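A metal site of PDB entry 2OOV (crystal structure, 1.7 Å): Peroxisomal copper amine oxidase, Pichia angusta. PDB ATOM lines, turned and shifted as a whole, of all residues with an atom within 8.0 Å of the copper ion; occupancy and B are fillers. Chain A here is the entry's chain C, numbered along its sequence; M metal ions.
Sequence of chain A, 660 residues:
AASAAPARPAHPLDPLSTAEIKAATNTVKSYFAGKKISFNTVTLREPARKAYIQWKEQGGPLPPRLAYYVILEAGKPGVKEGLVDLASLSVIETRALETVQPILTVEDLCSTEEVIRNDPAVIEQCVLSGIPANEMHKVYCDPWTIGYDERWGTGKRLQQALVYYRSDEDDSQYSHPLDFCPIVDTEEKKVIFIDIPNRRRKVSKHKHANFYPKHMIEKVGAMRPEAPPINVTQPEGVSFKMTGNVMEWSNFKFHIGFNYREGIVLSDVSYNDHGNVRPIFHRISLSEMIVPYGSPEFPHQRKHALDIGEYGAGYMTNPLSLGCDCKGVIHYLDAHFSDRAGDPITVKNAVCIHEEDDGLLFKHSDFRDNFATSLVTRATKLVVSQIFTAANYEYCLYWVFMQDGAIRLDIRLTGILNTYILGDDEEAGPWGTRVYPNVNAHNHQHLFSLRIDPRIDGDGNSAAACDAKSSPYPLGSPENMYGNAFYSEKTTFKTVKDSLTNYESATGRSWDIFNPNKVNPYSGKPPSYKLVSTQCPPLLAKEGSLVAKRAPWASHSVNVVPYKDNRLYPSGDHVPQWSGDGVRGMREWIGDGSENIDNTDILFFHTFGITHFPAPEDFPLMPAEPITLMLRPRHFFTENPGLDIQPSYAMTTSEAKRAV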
ATOM      1  N   VAL A 291       5.647 -17.272  17.400  1.00  0.00           N
ATOM      2  CA  VAL A 291       6.657 -18.114  16.731  1.00  0.00           C
ATOM      3  C   VAL A 291       6.822 -19.417  17.560  1.00  0.00           C
ATOM      4  O   VAL A 291       7.805 -19.585  18.312  1.00  0.00           O
ATOM      5  CB  VAL A 291       7.983 -17.325  16.516  1.00  0.00           C
ATOM      6  CG1 VAL A 291       9.071 -18.170  15.829  1.00  0.00           C
ATOM      7  CG2 VAL A 291       7.724 -16.079  15.678  1.00  0.00           C
ATOM      8  N   TYR A 293       7.707 -22.919  18.821  1.00  0.00           N
ATOM      9  CA  TYR A 293       8.630 -24.035  18.572  1.00  0.00           C
ATOM     10  C   TYR A 293       7.980 -25.402  18.807  1.00  0.00           C
ATOM     11  O   TYR A 293       7.008 -25.533  19.571  1.00  0.00           O
ATOM     12  CB  TYR A 293       9.967 -23.836  19.368  1.00  0.00           C
ATOM     13  CG  TYR A 293      10.876 -22.873  18.639  1.00  0.00           C
ATOM     14  CD1 TYR A 293      10.582 -21.487  18.594  1.00  0.00           C
ATOM     15  CD2 TYR A 293      11.998 -23.333  17.930  1.00  0.00           C
ATOM     16  CE1 TYR A 293      11.363 -20.609  17.878  1.00  0.00           C
ATOM     17  CE2 TYR A 293      12.784 -22.440  17.195  1.00  0.00           C
ATOM     18  CZ  TYR A 293      12.464 -21.078  17.187  1.00  0.00           C
ATOM     19  OH  TYR A 293      13.221 -20.180  16.459  1.00  0.00           O
ATOM     20  N   ASN A 392      18.105 -13.417  17.349  1.00  0.00           N
ATOM     21  CA  ASN A 392      18.673 -14.171  16.215  1.00  0.00           C
ATOM     22  C   ASN A 392      17.993 -13.872  14.865  1.00  0.00           C
ATOM     23  O   ASN A 392      18.677 -13.946  13.830  1.00  0.00           O
ATOM     24  CB  ASN A 392      18.621 -15.684  16.482  1.00  0.00           C
ATOM     25  CG  ASN A 392      17.224 -16.158  16.835  1.00  0.00           C
ATOM     26  OD1 ASN A 392      16.658 -15.772  17.862  1.00  0.00           O
ATOM     27  ND2 ASN A 392      16.639 -16.982  15.961  1.00  0.00           N
ATOM     28  N   TPQ A 393      16.754 -13.566  14.792  1.00  0.00           N
ATOM     29  CA  TPQ A 393      15.908 -13.441  13.588  1.00  0.00           C
ATOM     30  CB  TPQ A 393      14.412 -13.644  13.868  1.00  0.00           C
ATOM     31  C   TPQ A 393      16.027 -12.049  13.015  1.00  0.00           C
ATOM     32  O   TPQ A 393      15.803 -11.119  13.822  1.00  0.00           O
ATOM     33  C1  TPQ A 393      14.094 -14.789  14.803  1.00  0.00           C
ATOM     34  C2  TPQ A 393      13.865 -16.141  14.224  1.00  0.00           C
ATOM     35  O2  TPQ A 393      13.933 -16.324  12.879  1.00  0.00           O
ATOM     36  C3  TPQ A 393      13.558 -17.205  15.066  1.00  0.00           C
ATOM     37  C4  TPQ A 393      13.489 -16.991  16.431  1.00  0.00           C
ATOM     38  O4  TPQ A 393      13.195 -18.001  17.262  1.00  0.00           O
ATOM     39  C5  TPQ A 393      13.734 -15.645  17.010  1.00  0.00           C
ATOM     40  O5  TPQ A 393      13.657 -15.470  18.367  1.00  0.00           O
ATOM     41  C6  TPQ A 393      14.016 -14.583  16.180  1.00  0.00           C
ATOM     42  N   TYR A 395      13.229  -9.839  10.506  1.00  0.00           N
ATOM     43  CA  TYR A 395      11.960  -9.783   9.796  1.00  0.00           C
ATOM     44  C   TYR A 395      11.973  -8.548   8.915  1.00  0.00           C
ATOM     45  O   TYR A 395      12.028  -7.424   9.421  1.00  0.00           O
ATOM     46  CB  TYR A 395      10.783  -9.715  10.792  1.00  0.00           C
ATOM     47  CG  TYR A 395      10.596 -11.007  11.565  1.00  0.00           C
ATOM     48  CD1 TYR A 395      11.256 -11.223  12.777  1.00  0.00           C
ATOM     49  CD2 TYR A 395       9.782 -12.026  11.059  1.00  0.00           C
ATOM     50  CE1 TYR A 395      11.107 -12.427  13.481  1.00  0.00           C
ATOM     51  CE2 TYR A 395       9.608 -13.230  11.762  1.00  0.00           C
ATOM     52  CZ  TYR A 395      10.285 -13.415  12.966  1.00  0.00           C
ATOM     53  OH  TYR A 395      10.136 -14.582  13.663  1.00  0.00           O
ATOM     54  N   LEU A 413      12.005 -13.385   5.682  1.00  0.00           N
ATOM     55  CA  LEU A 413      12.595 -13.831   6.935  1.00  0.00           C
ATOM     56  C   LEU A 413      14.044 -14.151   6.660  1.00  0.00           C
ATOM     57  O   LEU A 413      14.338 -14.902   5.739  1.00  0.00           O
ATOM     58  CB  LEU A 413      11.921 -15.095   7.445  1.00  0.00           C
ATOM     59  CG  LEU A 413      10.409 -15.221   7.594  1.00  0.00           C
ATOM     60  CD1 LEU A 413      10.056 -16.549   8.264  1.00  0.00           C
ATOM     61  CD2 LEU A 413       9.861 -14.070   8.405  1.00  0.00           C
ATOM     62  N   THR A 414      14.937 -13.596   7.469  1.00  0.00           N
ATOM     63  CA  THR A 414      16.355 -13.970   7.362  1.00  0.00           C
ATOM     64  C   THR A 414      16.931 -13.941   8.785  1.00  0.00           C
ATOM     65  O   THR A 414      16.180 -14.056   9.761  1.00  0.00           O
ATOM     66  CB  THR A 414      17.120 -13.101   6.306  1.00  0.00           C
ATOM     67  OG1 THR A 414      18.500 -13.495   6.214  1.00  0.00           O
ATOM     68  CG2 THR A 414      17.020 -11.604   6.594  1.00  0.00           C
ATOM     69  N   ILE A 416      19.369 -15.688  11.722  1.00  0.00           N
ATOM     70  CA  ILE A 416      19.992 -16.943  12.156  1.00  0.00           C
ATOM     71  C   ILE A 416      18.978 -17.837  12.862  1.00  0.00           C
ATOM     72  O   ILE A 416      18.123 -17.351  13.622  1.00  0.00           O
ATOM     73  CB  ILE A 416      21.171 -16.616  13.123  1.00  0.00           C
ATOM     74  CG1 ILE A 416      22.190 -15.724  12.396  1.00  0.00           C
ATOM     75  CG2 ILE A 416      21.831 -17.925  13.623  1.00  0.00           C
ATOM     76  CD1 ILE A 416      23.367 -15.303  13.228  1.00  0.00           C
ATOM     77  N   LEU A 417      19.046 -19.132  12.593  1.00  0.00           N
ATOM     78  CA  LEU A 417      18.229 -20.114  13.295  1.00  0.00           C
ATOM     79  C   LEU A 417      18.440 -20.042  14.804  1.00  0.00           C
ATOM     80  O   LEU A 417      19.586 -19.926  15.277  1.00  0.00           O
ATOM     81  CB  LEU A 417      18.625 -21.536  12.851  1.00  0.00           C
ATOM     82  CG  LEU A 417      18.267 -21.932  11.420  1.00  0.00           C
ATOM     83  CD1 LEU A 417      19.001 -23.251  11.088  1.00  0.00           C
ATOM     84  CD2 LEU A 417      16.744 -22.105  11.265  1.00  0.00           C
ATOM     85  N   ASN A 418      17.354 -20.166  15.562  1.00  0.00           N
ATOM     86  CA  ASN A 418      17.497 -20.507  16.986  1.00  0.00           C
ATOM     87  C   ASN A 418      18.028 -21.930  17.076  1.00  0.00           C
ATOM     88  O   ASN A 418      17.494 -22.853  16.432  1.00  0.00           O
ATOM     89  CB  ASN A 418      16.156 -20.400  17.734  1.00  0.00           C
ATOM     90  CG  ASN A 418      16.149 -21.173  19.049  1.00  0.00           C
ATOM     91  OD1 ASN A 418      15.708 -22.332  19.104  1.00  0.00           O
ATOM     92  ND2 ASN A 418      16.661 -20.555  20.091  1.00  0.00           N
ATOM     93  N   HIS A 442      15.540 -26.429  16.191  1.00  0.00           N
ATOM     94  CA  HIS A 442      14.188 -26.951  16.417  1.00  0.00           C
ATOM     95  C   HIS A 442      13.157 -26.454  15.368  1.00  0.00           C
ATOM     96  O   HIS A 442      13.251 -25.317  14.878  1.00  0.00           O
ATOM     97  CB  HIS A 442      13.649 -26.559  17.805  1.00  0.00           C
ATOM     98  CG  HIS A 442      14.325 -27.243  18.949  1.00  0.00           C
ATOM     99  ND1 HIS A 442      14.526 -26.635  20.178  1.00  0.00           N
ATOM    100  CD2 HIS A 442      14.845 -28.494  19.062  1.00  0.00           C
ATOM    101  CE1 HIS A 442      15.139 -27.476  20.988  1.00  0.00           C
ATOM    102  NE2 HIS A 442      15.342 -28.617  20.345  1.00  0.00           N
ATOM    103  N   ASN A 443      12.196 -27.317  15.075  1.00  0.00           N
ATOM    104  CA  ASN A 443      11.061 -26.973  14.223  1.00  0.00           C
ATOM    105  C   ASN A 443      10.290 -25.824  14.854  1.00  0.00           C
ATOM    106  O   ASN A 443      10.221 -25.732  16.082  1.00  0.00           O
ATOM    107  CB  ASN A 443      10.088 -28.146  14.090  1.00  0.00           C
ATOM    108  CG  ASN A 443      10.719 -29.358  13.454  1.00  0.00           C
ATOM    109  OD1 ASN A 443      11.743 -29.273  12.785  1.00  0.00           O
ATOM    110  ND2 ASN A 443      10.063 -30.502  13.619  1.00  0.00           N
ATOM    111  N   HIS A 444       9.712 -24.956  14.022  1.00  0.00           N
ATOM    112  CA  HIS A 444       8.906 -23.835  14.545  1.00  0.00           C
ATOM    113  C   HIS A 444       8.052 -23.274  13.433  1.00  0.00           C
ATOM    114  O   HIS A 444       8.362 -23.464  12.260  1.00  0.00           O
ATOM    115  CB  HIS A 444       9.816 -22.722  15.117  1.00  0.00           C
ATOM    116  CG  HIS A 444      10.834 -22.223  14.125  1.00  0.00           C
ATOM    117  ND1 HIS A 444      11.975 -22.924  13.813  1.00  0.00           N
ATOM    118  CD2 HIS A 444      10.841 -21.110  13.338  1.00  0.00           C
ATOM    119  CE1 HIS A 444      12.645 -22.268  12.864  1.00  0.00           C
ATOM    120  NE2 HIS A 444      11.979 -21.166  12.572  1.00  0.00           N
ATOM    121  N   GLN A 445       6.973 -22.573  13.807  1.00  0.00           N
ATOM    122  CA  GLN A 445       6.159 -21.813  12.862  1.00  0.00           C
ATOM    123  C   GLN A 445       6.405 -20.324  13.099  1.00  0.00           C
ATOM    124  O   GLN A 445       6.746 -19.925  14.220  1.00  0.00           O
ATOM    125  CB  GLN A 445       4.686 -22.104  13.077  1.00  0.00           C
ATOM    126  CG  GLN A 445       4.314 -23.567  12.894  1.00  0.00           C
ATOM    127  CD  GLN A 445       2.804 -23.757  12.939  1.00  0.00           C
ATOM    128  OE1 GLN A 445       2.202 -23.764  14.029  1.00  0.00           O
ATOM    129  NE2 GLN A 445       2.192 -23.888  11.761  1.00  0.00           N
ATOM    130  N   HIS A 446       6.248 -19.511  12.053  1.00  0.00           N
ATOM    131  CA  HIS A 446       6.211 -18.060  12.237  1.00  0.00           C
ATOM    132  C   HIS A 446       4.802 -17.644  11.805  1.00  0.00           C
ATOM    133  O   HIS A 446       4.447 -17.810  10.631  1.00  0.00           O
ATOM    134  CB  HIS A 446       7.211 -17.324  11.330  1.00  0.00           C
ATOM    135  CG  HIS A 446       8.645 -17.739  11.490  1.00  0.00           C
ATOM    136  ND1 HIS A 446       9.552 -17.008  12.231  1.00  0.00           N
ATOM    137  CD2 HIS A 446       9.347 -18.754  10.936  1.00  0.00           C
ATOM    138  CE1 HIS A 446      10.742 -17.572  12.140  1.00  0.00           C
ATOM    139  NE2 HIS A 446      10.648 -18.634  11.356  1.00  0.00           N
ATOM    140  N   ILE A 610       4.401 -19.176   7.989  1.00  0.00           N
ATOM    141  CA  ILE A 610       5.086 -20.375   7.480  1.00  0.00           C
ATOM    142  C   ILE A 610       5.414 -21.380   8.582  1.00  0.00           C
ATOM    143  O   ILE A 610       5.440 -21.036   9.745  1.00  0.00           O
ATOM    144  CB  ILE A 610       6.411 -20.048   6.730  1.00  0.00           C
ATOM    145  CG1 ILE A 610       7.431 -19.416   7.697  1.00  0.00           C
ATOM    146  CG2 ILE A 610       6.151 -19.181   5.450  1.00  0.00           C
ATOM    147  CD1 ILE A 610       8.870 -19.713   7.325  1.00  0.00           C
ATOM    148  N   THR A 611       5.691 -22.623   8.184  1.00  0.00           N
ATOM    149  CA  THR A 611       6.124 -23.658   9.092  1.00  0.00           C
ATOM    150  C   THR A 611       7.533 -24.001   8.651  1.00  0.00           C
ATOM    151  O   THR A 611       7.759 -24.377   7.498  1.00  0.00           O
ATOM    152  CB  THR A 611       5.188 -24.862   8.999  1.00  0.00           C
ATOM    153  OG1 THR A 611       3.875 -24.437   9.409  1.00  0.00           O
ATOM    154  CG2 THR A 611       5.677 -25.999   9.921  1.00  0.00           C
ATOM    155  N   HIS A 612       8.485 -23.865   9.570  1.00  0.00           N
ATOM    156  CA  HIS A 612       9.892 -23.943   9.220  1.00  0.00           C
ATOM    157  C   HIS A 612      10.496 -25.220   9.772  1.00  0.00           C
ATOM    158  O   HIS A 612      10.558 -25.425  10.991  1.00  0.00           O
ATOM    159  CB  HIS A 612      10.606 -22.709   9.801  1.00  0.00           C
ATOM    160  CG  HIS A 612      12.033 -22.544   9.373  1.00  0.00           C
ATOM    161  ND1 HIS A 612      12.784 -21.444   9.716  1.00  0.00           N
ATOM    162  CD2 HIS A 612      12.836 -23.330   8.614  1.00  0.00           C
ATOM    163  CE1 HIS A 612      14.003 -21.566   9.217  1.00  0.00           C
ATOM    164  NE2 HIS A 612      14.062 -22.700   8.537  1.00  0.00           N
ATOM    165  N   PHE A 613      10.910 -26.096   8.865  1.00  0.00           N
ATOM    166  CA  PHE A 613      11.677 -27.293   9.233  1.00  0.00           C
ATOM    167  C   PHE A 613      13.111 -27.038   8.756  1.00  0.00           C
ATOM    168  O   PHE A 613      13.409 -27.127   7.543  1.00  0.00           O
ATOM    169  CB  PHE A 613      11.084 -28.531   8.544  1.00  0.00           C
ATOM    170  CG  PHE A 613       9.673 -28.841   8.961  1.00  0.00           C
ATOM    171  CD1 PHE A 613       9.412 -29.469  10.186  1.00  0.00           C
ATOM    172  CD2 PHE A 613       8.607 -28.561   8.109  1.00  0.00           C
ATOM    173  CE1 PHE A 613       8.100 -29.775  10.582  1.00  0.00           C
ATOM    174  CE2 PHE A 613       7.275 -28.853   8.499  1.00  0.00           C
ATOM    175  CZ  PHE A 613       7.034 -29.460   9.736  1.00  0.00           C
ATOM    176  N   PRO A 614      13.995 -26.647   9.695  1.00  0.00           N
ATOM    177  CA  PRO A 614      15.344 -26.221   9.315  1.00  0.00           C
ATOM    178  C   PRO A 614      16.091 -27.248   8.496  1.00  0.00           C
ATOM    179  O   PRO A 614      15.874 -28.451   8.628  1.00  0.00           O
ATOM    180  CB  PRO A 614      16.028 -25.976  10.675  1.00  0.00           C
ATOM    181  CG  PRO A 614      14.854 -25.542  11.564  1.00  0.00           C
ATOM    182  CD  PRO A 614      13.776 -26.526  11.156  1.00  0.00           C
ATOM    183  N   ASP A 618      20.024 -23.341   5.760  1.00  0.00           N
ATOM    184  CA  ASP A 618      19.588 -22.219   6.602  1.00  0.00           C
ATOM    185  C   ASP A 618      20.697 -21.730   7.550  1.00  0.00           C
ATOM    186  O   ASP A 618      20.534 -20.715   8.238  1.00  0.00           O
ATOM    187  CB  ASP A 618      18.409 -22.650   7.473  1.00  0.00           C
ATOM    188  CG  ASP A 618      17.150 -22.993   6.664  1.00  0.00           C
ATOM    189  OD1 ASP A 618      16.980 -22.525   5.513  1.00  0.00           O
ATOM    190  OD2 ASP A 618      16.315 -23.733   7.228  1.00  0.00           O
ATOM    191  N   MET A 622      20.706 -17.571   7.376  1.00  0.00           N
ATOM    192  CA  MET A 622      19.679 -18.103   6.476  1.00  0.00           C
ATOM    193  C   MET A 622      19.315 -17.219   5.294  1.00  0.00           C
ATOM    194  O   MET A 622      19.059 -16.036   5.466  1.00  0.00           O
ATOM    195  CB  MET A 622      18.430 -18.560   7.230  1.00  0.00           C
ATOM    196  CG  MET A 622      17.603 -17.466   7.834  1.00  0.00           C
ATOM    197  SD  MET A 622      16.163 -18.181   8.652  1.00  0.00           S
ATOM    198  CE  MET A 622      14.999 -18.259   7.277  1.00  0.00           C
ATOM    199  N   GLU A 625      13.526 -16.011   3.238  1.00  0.00           N
ATOM    200  CA  GLU A 625      12.358 -16.837   2.932  1.00  0.00           C
ATOM    201  C   GLU A 625      11.132 -15.911   2.804  1.00  0.00           C
ATOM    202  O   GLU A 625      10.825 -15.145   3.734  1.00  0.00           O
ATOM    203  CB  GLU A 625      12.093 -17.902   4.007  1.00  0.00           C
ATOM    204  CG  GLU A 625      10.871 -18.742   3.651  1.00  0.00           C
ATOM    205  CD  GLU A 625      10.762 -20.055   4.404  1.00  0.00           C
ATOM    206  OE1 GLU A 625      11.645 -20.366   5.231  1.00  0.00           O
ATOM    207  OE2 GLU A 625       9.759 -20.763   4.164  1.00  0.00           O
HETATM  208 CU    CU M   1      12.044 -20.007  10.897  1.00  0.00          CU
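Of the 23 residues printed, 3 come within 4 Å of the copper ion.
A ring nitrogen (ND1) of His 446 lies within hydrogen-bond range of the side-chain hydroxyl of Tyr 395.
The backbone NH of His 446 lies within hydrogen-bond range of the backbone carbonyl oxygen of Ile 610 (2.9 Å).
The side-chain carboxylate (OD2) of Asp 618 lies within hydrogen-bond range of a ring nitrogen (NE2) of His 612, 2.8 Å away.
ND1 of His 444 lies within hydrogen-bond range of O of His 442.
ND1 of His 612 binds the copper ion (2.0 Å).
NE2 of His 446 is bound to the copper ion (2.0 Å).
A ring nitrogen (NE2) of His 444 is bound to the copper ion, 2.0 Å away.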
